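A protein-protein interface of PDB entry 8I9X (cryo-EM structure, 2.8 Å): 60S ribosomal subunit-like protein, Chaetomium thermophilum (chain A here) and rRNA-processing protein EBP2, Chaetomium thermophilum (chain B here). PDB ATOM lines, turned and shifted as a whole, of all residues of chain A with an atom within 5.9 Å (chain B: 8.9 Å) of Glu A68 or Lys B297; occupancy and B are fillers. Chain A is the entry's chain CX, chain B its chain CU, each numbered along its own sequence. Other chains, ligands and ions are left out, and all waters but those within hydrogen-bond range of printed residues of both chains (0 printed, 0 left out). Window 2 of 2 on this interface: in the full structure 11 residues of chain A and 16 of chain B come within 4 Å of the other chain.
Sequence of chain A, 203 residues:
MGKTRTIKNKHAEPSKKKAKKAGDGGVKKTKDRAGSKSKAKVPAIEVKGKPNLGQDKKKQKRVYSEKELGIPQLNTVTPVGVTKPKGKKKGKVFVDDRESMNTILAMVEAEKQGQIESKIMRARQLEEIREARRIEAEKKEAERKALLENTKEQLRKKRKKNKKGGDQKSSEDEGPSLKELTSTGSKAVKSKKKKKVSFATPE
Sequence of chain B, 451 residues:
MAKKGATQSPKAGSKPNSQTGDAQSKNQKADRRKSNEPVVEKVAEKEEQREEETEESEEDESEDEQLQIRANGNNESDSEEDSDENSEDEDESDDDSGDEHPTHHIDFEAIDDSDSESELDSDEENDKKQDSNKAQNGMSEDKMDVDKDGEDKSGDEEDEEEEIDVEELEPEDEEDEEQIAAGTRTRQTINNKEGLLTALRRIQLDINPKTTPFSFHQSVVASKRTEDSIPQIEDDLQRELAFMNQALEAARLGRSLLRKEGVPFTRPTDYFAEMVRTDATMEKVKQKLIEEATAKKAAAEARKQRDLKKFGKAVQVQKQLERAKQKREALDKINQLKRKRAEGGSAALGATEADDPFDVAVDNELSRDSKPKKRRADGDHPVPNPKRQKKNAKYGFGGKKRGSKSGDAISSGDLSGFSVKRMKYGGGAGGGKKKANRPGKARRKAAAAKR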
ATOM      1  N   VAL A  63     -19.000 -10.072  24.268  1.00  0.00           N
ATOM      2  CA  VAL A  63     -17.596 -10.271  24.598  1.00  0.00           C
ATOM      3  C   VAL A  63     -17.318 -11.749  24.837  1.00  0.00           C
ATOM      4  O   VAL A  63     -18.000 -12.397  25.630  1.00  0.00           O
ATOM      5  CB  VAL A  63     -17.187  -9.435  25.823  1.00  0.00           C
ATOM      6  CG1 VAL A  63     -15.697  -9.581  26.092  1.00  0.00           C
ATOM      7  CG2 VAL A  63     -17.557  -7.974  25.613  1.00  0.00           C
ATOM      8  N   TYR A  64     -16.310 -12.277  24.147  1.00  0.00           N
ATOM      9  CA  TYR A  64     -15.922 -13.676  24.251  1.00  0.00           C
ATOM     10  C   TYR A  64     -14.420 -13.759  24.478  1.00  0.00           C
ATOM     11  O   TYR A  64     -13.666 -12.913  23.986  1.00  0.00           O
ATOM     12  CB  TYR A  64     -16.323 -14.451  22.996  1.00  0.00           C
ATOM     13  CG  TYR A  64     -17.732 -14.159  22.531  1.00  0.00           C
ATOM     14  CD1 TYR A  64     -18.819 -14.382  23.365  1.00  0.00           C
ATOM     15  CD2 TYR A  64     -17.975 -13.657  21.260  1.00  0.00           C
ATOM     16  CE1 TYR A  64     -20.109 -14.115  22.945  1.00  0.00           C
ATOM     17  CE2 TYR A  64     -19.260 -13.388  20.830  1.00  0.00           C
ATOM     18  CZ  TYR A  64     -20.324 -13.619  21.678  1.00  0.00           C
ATOM     19  OH  TYR A  64     -21.605 -13.351  21.255  1.00  0.00           O
ATOM     20  N   SER A  65     -13.991 -14.777  25.223  1.00  0.00           N
ATOM     21  CA  SER A  65     -12.601 -14.861  25.647  1.00  0.00           C
ATOM     22  C   SER A  65     -11.694 -15.279  24.496  1.00  0.00           C
ATOM     23  O   SER A  65     -12.060 -16.092  23.639  1.00  0.00           O
ATOM     24  CB  SER A  65     -12.459 -15.843  26.812  1.00  0.00           C
ATOM     25  OG  SER A  65     -13.139 -17.056  26.545  1.00  0.00           O
ATOM     26  N   GLU A  66     -10.489 -14.707  24.489  1.00  0.00           N
ATOM     27  CA  GLU A  66      -9.448 -15.070  23.539  1.00  0.00           C
ATOM     28  C   GLU A  66      -8.989 -16.511  23.700  1.00  0.00           C
ATOM     29  O   GLU A  66      -8.424 -17.071  22.756  1.00  0.00           O
ATOM     30  CB  GLU A  66      -8.249 -14.131  23.691  1.00  0.00           C
ATOM     31  CG  GLU A  66      -8.494 -12.718  23.192  1.00  0.00           C
ATOM     32  CD  GLU A  66      -8.019 -11.662  24.169  1.00  0.00           C
ATOM     33  OE1 GLU A  66      -7.399 -12.028  25.189  1.00  0.00           O
ATOM     34  OE2 GLU A  66      -8.264 -10.463  23.916  1.00  0.00           O
ATOM     35  N   LYS A  67      -9.197 -17.112  24.871  1.00  0.00           N
ATOM     36  CA  LYS A  67      -8.917 -18.532  25.037  1.00  0.00           C
ATOM     37  C   LYS A  67      -9.980 -19.382  24.354  1.00  0.00           C
ATOM     38  O   LYS A  67      -9.658 -20.400  23.729  1.00  0.00           O
ATOM     39  CB  LYS A  67      -8.816 -18.874  26.525  1.00  0.00           C
ATOM     40  CG  LYS A  67      -8.569 -20.347  26.831  1.00  0.00           C
ATOM     41  CD  LYS A  67      -9.852 -21.063  27.232  1.00  0.00           C
ATOM     42  CE  LYS A  67     -10.337 -20.604  28.597  1.00  0.00           C
ATOM     43  NZ  LYS A  67     -11.580 -21.310  29.012  1.00  0.00           N
ATOM     44  N   GLU A  68     -11.246 -18.983  24.463  1.00  0.00           N
ATOM     45  CA  GLU A  68     -12.332 -19.693  23.800  1.00  0.00           C
ATOM     46  C   GLU A  68     -12.179 -19.594  22.289  1.00  0.00           C
ATOM     47  O   GLU A  68     -12.242 -20.607  21.585  1.00  0.00           O
ATOM     48  CB  GLU A  68     -13.688 -19.140  24.240  1.00  0.00           C
ATOM     49  CG  GLU A  68     -14.809 -19.363  23.241  1.00  0.00           C
ATOM     50  CD  GLU A  68     -16.105 -18.702  23.667  1.00  0.00           C
ATOM     51  OE1 GLU A  68     -16.066 -17.847  24.576  1.00  0.00           O
ATOM     52  OE2 GLU A  68     -17.162 -19.041  23.095  1.00  0.00           O
ATOM     53  N   LEU A  69     -11.976 -18.380  21.783  1.00  0.00           N
ATOM     54  CA  LEU A  69     -11.721 -18.214  20.358  1.00  0.00           C
ATOM     55  C   LEU A  69     -10.351 -18.778  20.003  1.00  0.00           C
ATOM     56  O   LEU A  69      -9.381 -18.600  20.743  1.00  0.00           O
ATOM     57  CB  LEU A  69     -11.807 -16.740  19.970  1.00  0.00           C
ATOM     58  CG  LEU A  69     -13.170 -16.074  20.154  1.00  0.00           C
ATOM     59  CD1 LEU A  69     -13.101 -14.603  19.783  1.00  0.00           C
ATOM     60  CD2 LEU A  69     -14.228 -16.789  19.332  1.00  0.00           C
ATOM     61  N   GLY A  70     -10.274 -19.466  18.869  1.00  0.00           N
ATOM     62  CA  GLY A  70      -9.014 -20.035  18.432  1.00  0.00           C
ATOM     63  C   GLY A  70      -8.083 -19.000  17.838  1.00  0.00           C
ATOM     64  O   GLY A  70      -7.741 -19.069  16.653  1.00  0.00           O
ATOM     65  N   ILE B 290      -9.940 -11.265  16.269  1.00  0.00           N
ATOM     66  CA  ILE B 290     -11.009 -11.353  17.260  1.00  0.00           C
ATOM     67  C   ILE B 290     -12.361 -11.102  16.609  1.00  0.00           C
ATOM     68  O   ILE B 290     -13.324 -11.835  16.850  1.00  0.00           O
ATOM     69  CB  ILE B 290     -10.758 -10.369  18.418  1.00  0.00           C
ATOM     70  CG1 ILE B 290      -9.481 -10.729  19.172  1.00  0.00           C
ATOM     71  CG2 ILE B 290     -11.948 -10.344  19.367  1.00  0.00           C
ATOM     72  CD1 ILE B 290      -9.550 -12.053  19.862  1.00  0.00           C
ATOM     73  N   GLU B 291     -12.456 -10.062  15.779  1.00  0.00           N
ATOM     74  CA  GLU B 291     -13.752  -9.728  15.197  1.00  0.00           C
ATOM     75  C   GLU B 291     -14.195 -10.783  14.190  1.00  0.00           C
ATOM     76  O   GLU B 291     -15.385 -11.101  14.105  1.00  0.00           O
ATOM     77  CB  GLU B 291     -13.726  -8.335  14.561  1.00  0.00           C
ATOM     78  CG  GLU B 291     -12.828  -8.170  13.357  1.00  0.00           C
ATOM     79  CD  GLU B 291     -12.834  -6.747  12.827  1.00  0.00           C
ATOM     80  OE1 GLU B 291     -13.527  -5.895  13.421  1.00  0.00           O
ATOM     81  OE2 GLU B 291     -12.152  -6.481  11.816  1.00  0.00           O
ATOM     82  N   GLU B 292     -13.256 -11.354  13.430  1.00  0.00           N
ATOM     83  CA  GLU B 292     -13.620 -12.419  12.499  1.00  0.00           C
ATOM     84  C   GLU B 292     -14.140 -13.649  13.237  1.00  0.00           C
ATOM     85  O   GLU B 292     -15.200 -14.196  12.887  1.00  0.00           O
ATOM     86  CB  GLU B 292     -12.420 -12.785  11.628  1.00  0.00           C
ATOM     87  CG  GLU B 292     -12.393 -12.086  10.280  1.00  0.00           C
ATOM     88  CD  GLU B 292     -11.169 -12.444   9.459  1.00  0.00           C
ATOM     89  OE1 GLU B 292     -10.270 -13.126   9.994  1.00  0.00           O
ATOM     90  OE2 GLU B 292     -11.107 -12.043   8.278  1.00  0.00           O
ATOM     91  N   ALA B 293     -13.416 -14.094  14.269  1.00  0.00           N
ATOM     92  CA  ALA B 293     -13.871 -15.247  15.039  1.00  0.00           C
ATOM     93  C   ALA B 293     -15.198 -14.959  15.732  1.00  0.00           C
ATOM     94  O   ALA B 293     -16.076 -15.832  15.798  1.00  0.00           O
ATOM     95  CB  ALA B 293     -12.808 -15.652  16.058  1.00  0.00           C
ATOM     96  N   THR B 294     -15.360 -13.742  16.255  1.00  0.00           N
ATOM     97  CA  THR B 294     -16.606 -13.364  16.906  1.00  0.00           C
ATOM     98  C   THR B 294     -17.766 -13.392  15.924  1.00  0.00           C
ATOM     99  O   THR B 294     -18.853 -13.868  16.258  1.00  0.00           O
ATOM    100  CB  THR B 294     -16.470 -11.978  17.537  1.00  0.00           C
ATOM    101  OG1 THR B 294     -15.456 -12.009  18.548  1.00  0.00           O
ATOM    102  CG2 THR B 294     -17.782 -11.542  18.163  1.00  0.00           C
ATOM    103  N   ALA B 295     -17.553 -12.897  14.703  1.00  0.00           N
ATOM    104  CA  ALA B 295     -18.611 -12.920  13.700  1.00  0.00           C
ATOM    105  C   ALA B 295     -19.005 -14.349  13.353  1.00  0.00           C
ATOM    106  O   ALA B 295     -20.196 -14.670  13.247  1.00  0.00           O
ATOM    107  CB  ALA B 295     -18.163 -12.164  12.450  1.00  0.00           C
ATOM    108  N   LYS B 296     -18.017 -15.229  13.185  1.00  0.00           N
ATOM    109  CA  LYS B 296     -18.340 -16.614  12.847  1.00  0.00           C
ATOM    110  C   LYS B 296     -19.112 -17.305  13.969  1.00  0.00           C
ATOM    111  O   LYS B 296     -20.160 -17.930  13.722  1.00  0.00           O
ATOM    112  CB  LYS B 296     -17.059 -17.381  12.521  1.00  0.00           C
ATOM    113  CG  LYS B 296     -17.279 -18.811  12.071  1.00  0.00           C
ATOM    114  CD  LYS B 296     -15.962 -19.480  11.717  1.00  0.00           C
ATOM    115  CE  LYS B 296     -16.183 -20.882  11.175  1.00  0.00           C
ATOM    116  NZ  LYS B 296     -16.707 -21.804  12.220  1.00  0.00           N
ATOM    117  N   LYS B 297     -18.635 -17.182  15.209  1.00  0.00           N
ATOM    118  CA  LYS B 297     -19.326 -17.831  16.318  1.00  0.00           C
ATOM    119  C   LYS B 297     -20.687 -17.189  16.567  1.00  0.00           C
ATOM    120  O   LYS B 297     -21.628 -17.863  17.003  1.00  0.00           O
ATOM    121  CB  LYS B 297     -18.451 -17.790  17.570  1.00  0.00           C
ATOM    122  CG  LYS B 297     -19.052 -18.478  18.782  1.00  0.00           C
ATOM    123  CD  LYS B 297     -18.061 -18.520  19.931  1.00  0.00           C
ATOM    124  CE  LYS B 297     -17.864 -17.143  20.535  1.00  0.00           C
ATOM    125  NZ  LYS B 297     -19.093 -16.685  21.233  1.00  0.00           N
ATOM    126  N   ALA B 298     -20.823 -15.897  16.259  1.00  0.00           N
ATOM    127  CA  ALA B 298     -22.110 -15.229  16.399  1.00  0.00           C
ATOM    128  C   ALA B 298     -23.108 -15.743  15.374  1.00  0.00           C
ATOM    129  O   ALA B 298     -24.293 -15.899  15.680  1.00  0.00           O
ATOM    130  CB  ALA B 298     -21.933 -13.718  16.267  1.00  0.00           C
ATOM    131  N   ALA B 299     -22.652 -16.007  14.149  1.00  0.00           N
ATOM    132  CA  ALA B 299     -23.528 -16.620  13.156  1.00  0.00           C
ATOM    133  C   ALA B 299     -23.974 -18.007  13.607  1.00  0.00           C
ATOM    134  O   ALA B 299     -25.136 -18.399  13.421  1.00  0.00           O
ATOM    135  CB  ALA B 299     -22.820 -16.691  11.802  1.00  0.00           C
ATOM    136  N   ALA B 300     -23.050 -18.770  14.198  1.00  0.00           N
ATOM    137  CA  ALA B 300     -23.419 -20.082  14.728  1.00  0.00           C
ATOM    138  C   ALA B 300     -24.489 -19.960  15.811  1.00  0.00           C
ATOM    139  O   ALA B 300     -25.505 -20.672  15.789  1.00  0.00           O
ATOM    140  CB  ALA B 300     -22.179 -20.796  15.266  1.00  0.00           C
ATOM    141  N   GLU B 301     -24.278 -19.051  16.767  1.00  0.00           N
ATOM    142  CA  GLU B 301     -25.274 -18.816  17.806  1.00  0.00           C
ATOM    143  C   GLU B 301     -26.598 -18.365  17.208  1.00  0.00           C
ATOM    144  O   GLU B 301     -27.670 -18.728  17.704  1.00  0.00           O
ATOM    145  CB  GLU B 301     -24.767 -17.776  18.807  1.00  0.00           C
ATOM    146  CG  GLU B 301     -23.473 -18.150  19.509  1.00  0.00           C
ATOM    147  CD  GLU B 301     -23.346 -17.500  20.873  1.00  0.00           C
ATOM    148  OE1 GLU B 301     -23.783 -16.339  21.022  1.00  0.00           O
ATOM    149  OE2 GLU B 301     -22.809 -18.149  21.796  1.00  0.00           O
ATOM    150  N   ALA B 302     -26.541 -17.575  16.136  1.00  0.00           N
ATOM    151  CA  ALA B 302     -27.755 -17.077  15.501  1.00  0.00           C
ATOM    152  C   ALA B 302     -28.584 -18.216  14.927  1.00  0.00           C
ATOM    153  O   ALA B 302     -29.801 -18.281  15.142  1.00  0.00           O
ATOM    154  CB  ALA B 302     -27.392 -16.073  14.409  1.00  0.00           C
ATOM    155  N   ARG B 303     -27.947 -19.121  14.183  1.00  0.00           N
ATOM    156  CA  ARG B 303     -28.705 -20.232  13.610  1.00  0.00           C
ATOM    157  C   ARG B 303     -29.241 -21.152  14.705  1.00  0.00           C
ATOM    158  O   ARG B 303     -30.390 -21.619  14.639  1.00  0.00           O
ATOM    159  CB  ARG B 303     -27.864 -21.006  12.589  1.00  0.00           C
ATOM    160  CG  ARG B 303     -26.643 -21.723  13.125  1.00  0.00           C
ATOM    161  CD  ARG B 303     -26.009 -22.580  12.038  1.00  0.00           C
ATOM    162  NE  ARG B 303     -25.557 -21.789  10.899  1.00  0.00           N
ATOM    163  CZ  ARG B 303     -24.353 -21.244  10.792  1.00  0.00           C
ATOM    164  NH1 ARG B 303     -23.436 -21.405  11.730  1.00  0.00           N
ATOM    165  NH2 ARG B 303     -24.059 -20.527   9.711  1.00  0.00           N
ATOM    166  N   LYS B 304     -28.434 -21.403  15.744  1.00  0.00           N
ATOM    167  CA  LYS B 304     -28.910 -22.240  16.841  1.00  0.00           C
ATOM    168  C   LYS B 304     -30.115 -21.611  17.530  1.00  0.00           C
ATOM    169  O   LYS B 304     -31.087 -22.299  17.865  1.00  0.00           O
ATOM    170  CB  LYS B 304     -27.785 -22.492  17.844  1.00  0.00           C
ATOM    171  CG  LYS B 304     -26.591 -23.232  17.270  1.00  0.00           C
ATOM    172  CD  LYS B 304     -26.954 -24.660  16.903  1.00  0.00           C
ATOM    173  CE  LYS B 304     -25.742 -25.426  16.401  1.00  0.00           C
ATOM    174  NZ  LYS B 304     -26.094 -26.815  15.997  1.00  0.00           N
ATOM    175  N   GLN B 305     -30.081 -20.294  17.735  1.00  0.00           N
ATOM    176  CA  GLN B 305     -31.164 -19.636  18.451  1.00  0.00           C
ATOM    177  C   GLN B 305     -32.412 -19.535  17.585  1.00  0.00           C
ATOM    178  O   GLN B 305     -33.534 -19.585  18.105  1.00  0.00           O
ATOM    179  CB  GLN B 305     -30.695 -18.261  18.928  1.00  0.00           C
ATOM    180  CG  GLN B 305     -31.491 -17.670  20.081  1.00  0.00           C
ATOM    181  CD  GLN B 305     -32.524 -16.655  19.647  1.00  0.00           C
ATOM    182  OE1 GLN B 305     -32.324 -15.920  18.681  1.00  0.00           O
ATOM    183  NE2 GLN B 305     -33.625 -16.586  20.383  1.00  0.00           N
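Among the printed residues, pairs that only touch across the chains: Tyr A64 with Thr B294, Tyr A64 with Lys B297, Tyr A64 with Glu B301, Glu A66 with Ile B290, Leu A69 with Ala B293, Leu A69 with Thr B294 and Leu A69 with Lys B297.
No residue of chain B comes within 4 Å of Ser A65. Glu A68 touches just one residue of chain B: Lys B297. Of the printed residues of chain B, Leu A69 touches Ala B293 (3.7 Å), Thr B294 (3.7 Å) and Lys B297 (3.8 Å). Printed residues of chain A within 4 Å of Ile B290: Glu A66. Of the printed residues of chain A, Thr B294 touches Tyr A64 and Leu A69. Of chain A, only Tyr A64 (3.1 Å), Glu A68 (3.3 Å) and Leu A69 (3.8 Å) come within 4 Å of Lys B297. The nearest residue of chain B that does not touch Glu A68 is Glu B301 (5.9 Å).
Of the 16 printed residues of chain B, 5 touch a printed residue of chain A. Hydrophobic or aromatic side chains of chain B within 4 Å of the printed part of chain A: Ile B290 and Ala B293. Of the 8 printed residues of chain A, 4 touch a printed residue of chain B. Among the printed residues, 8 pairs touch across the chains. Among the printed residues, Asp or Glu carboxylates within 4 Å of a Lys or Arg side-chain nitrogen of the other chain: Glu A68 with Lys B297.
The backbone carbonyl oxygen (O) of Ile B290 sits at hydrogen-bond distance from the side-chain hydroxyl (OG1) of Thr B294, 2.7 Å away. The backbone NH of Glu A68 lies close to the side-chain hydroxyl of Ser A65 (3.4 Å).
NZ of Lys B297 is in salt-bridge range of OE2 of Glu A68 (3.6 Å).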
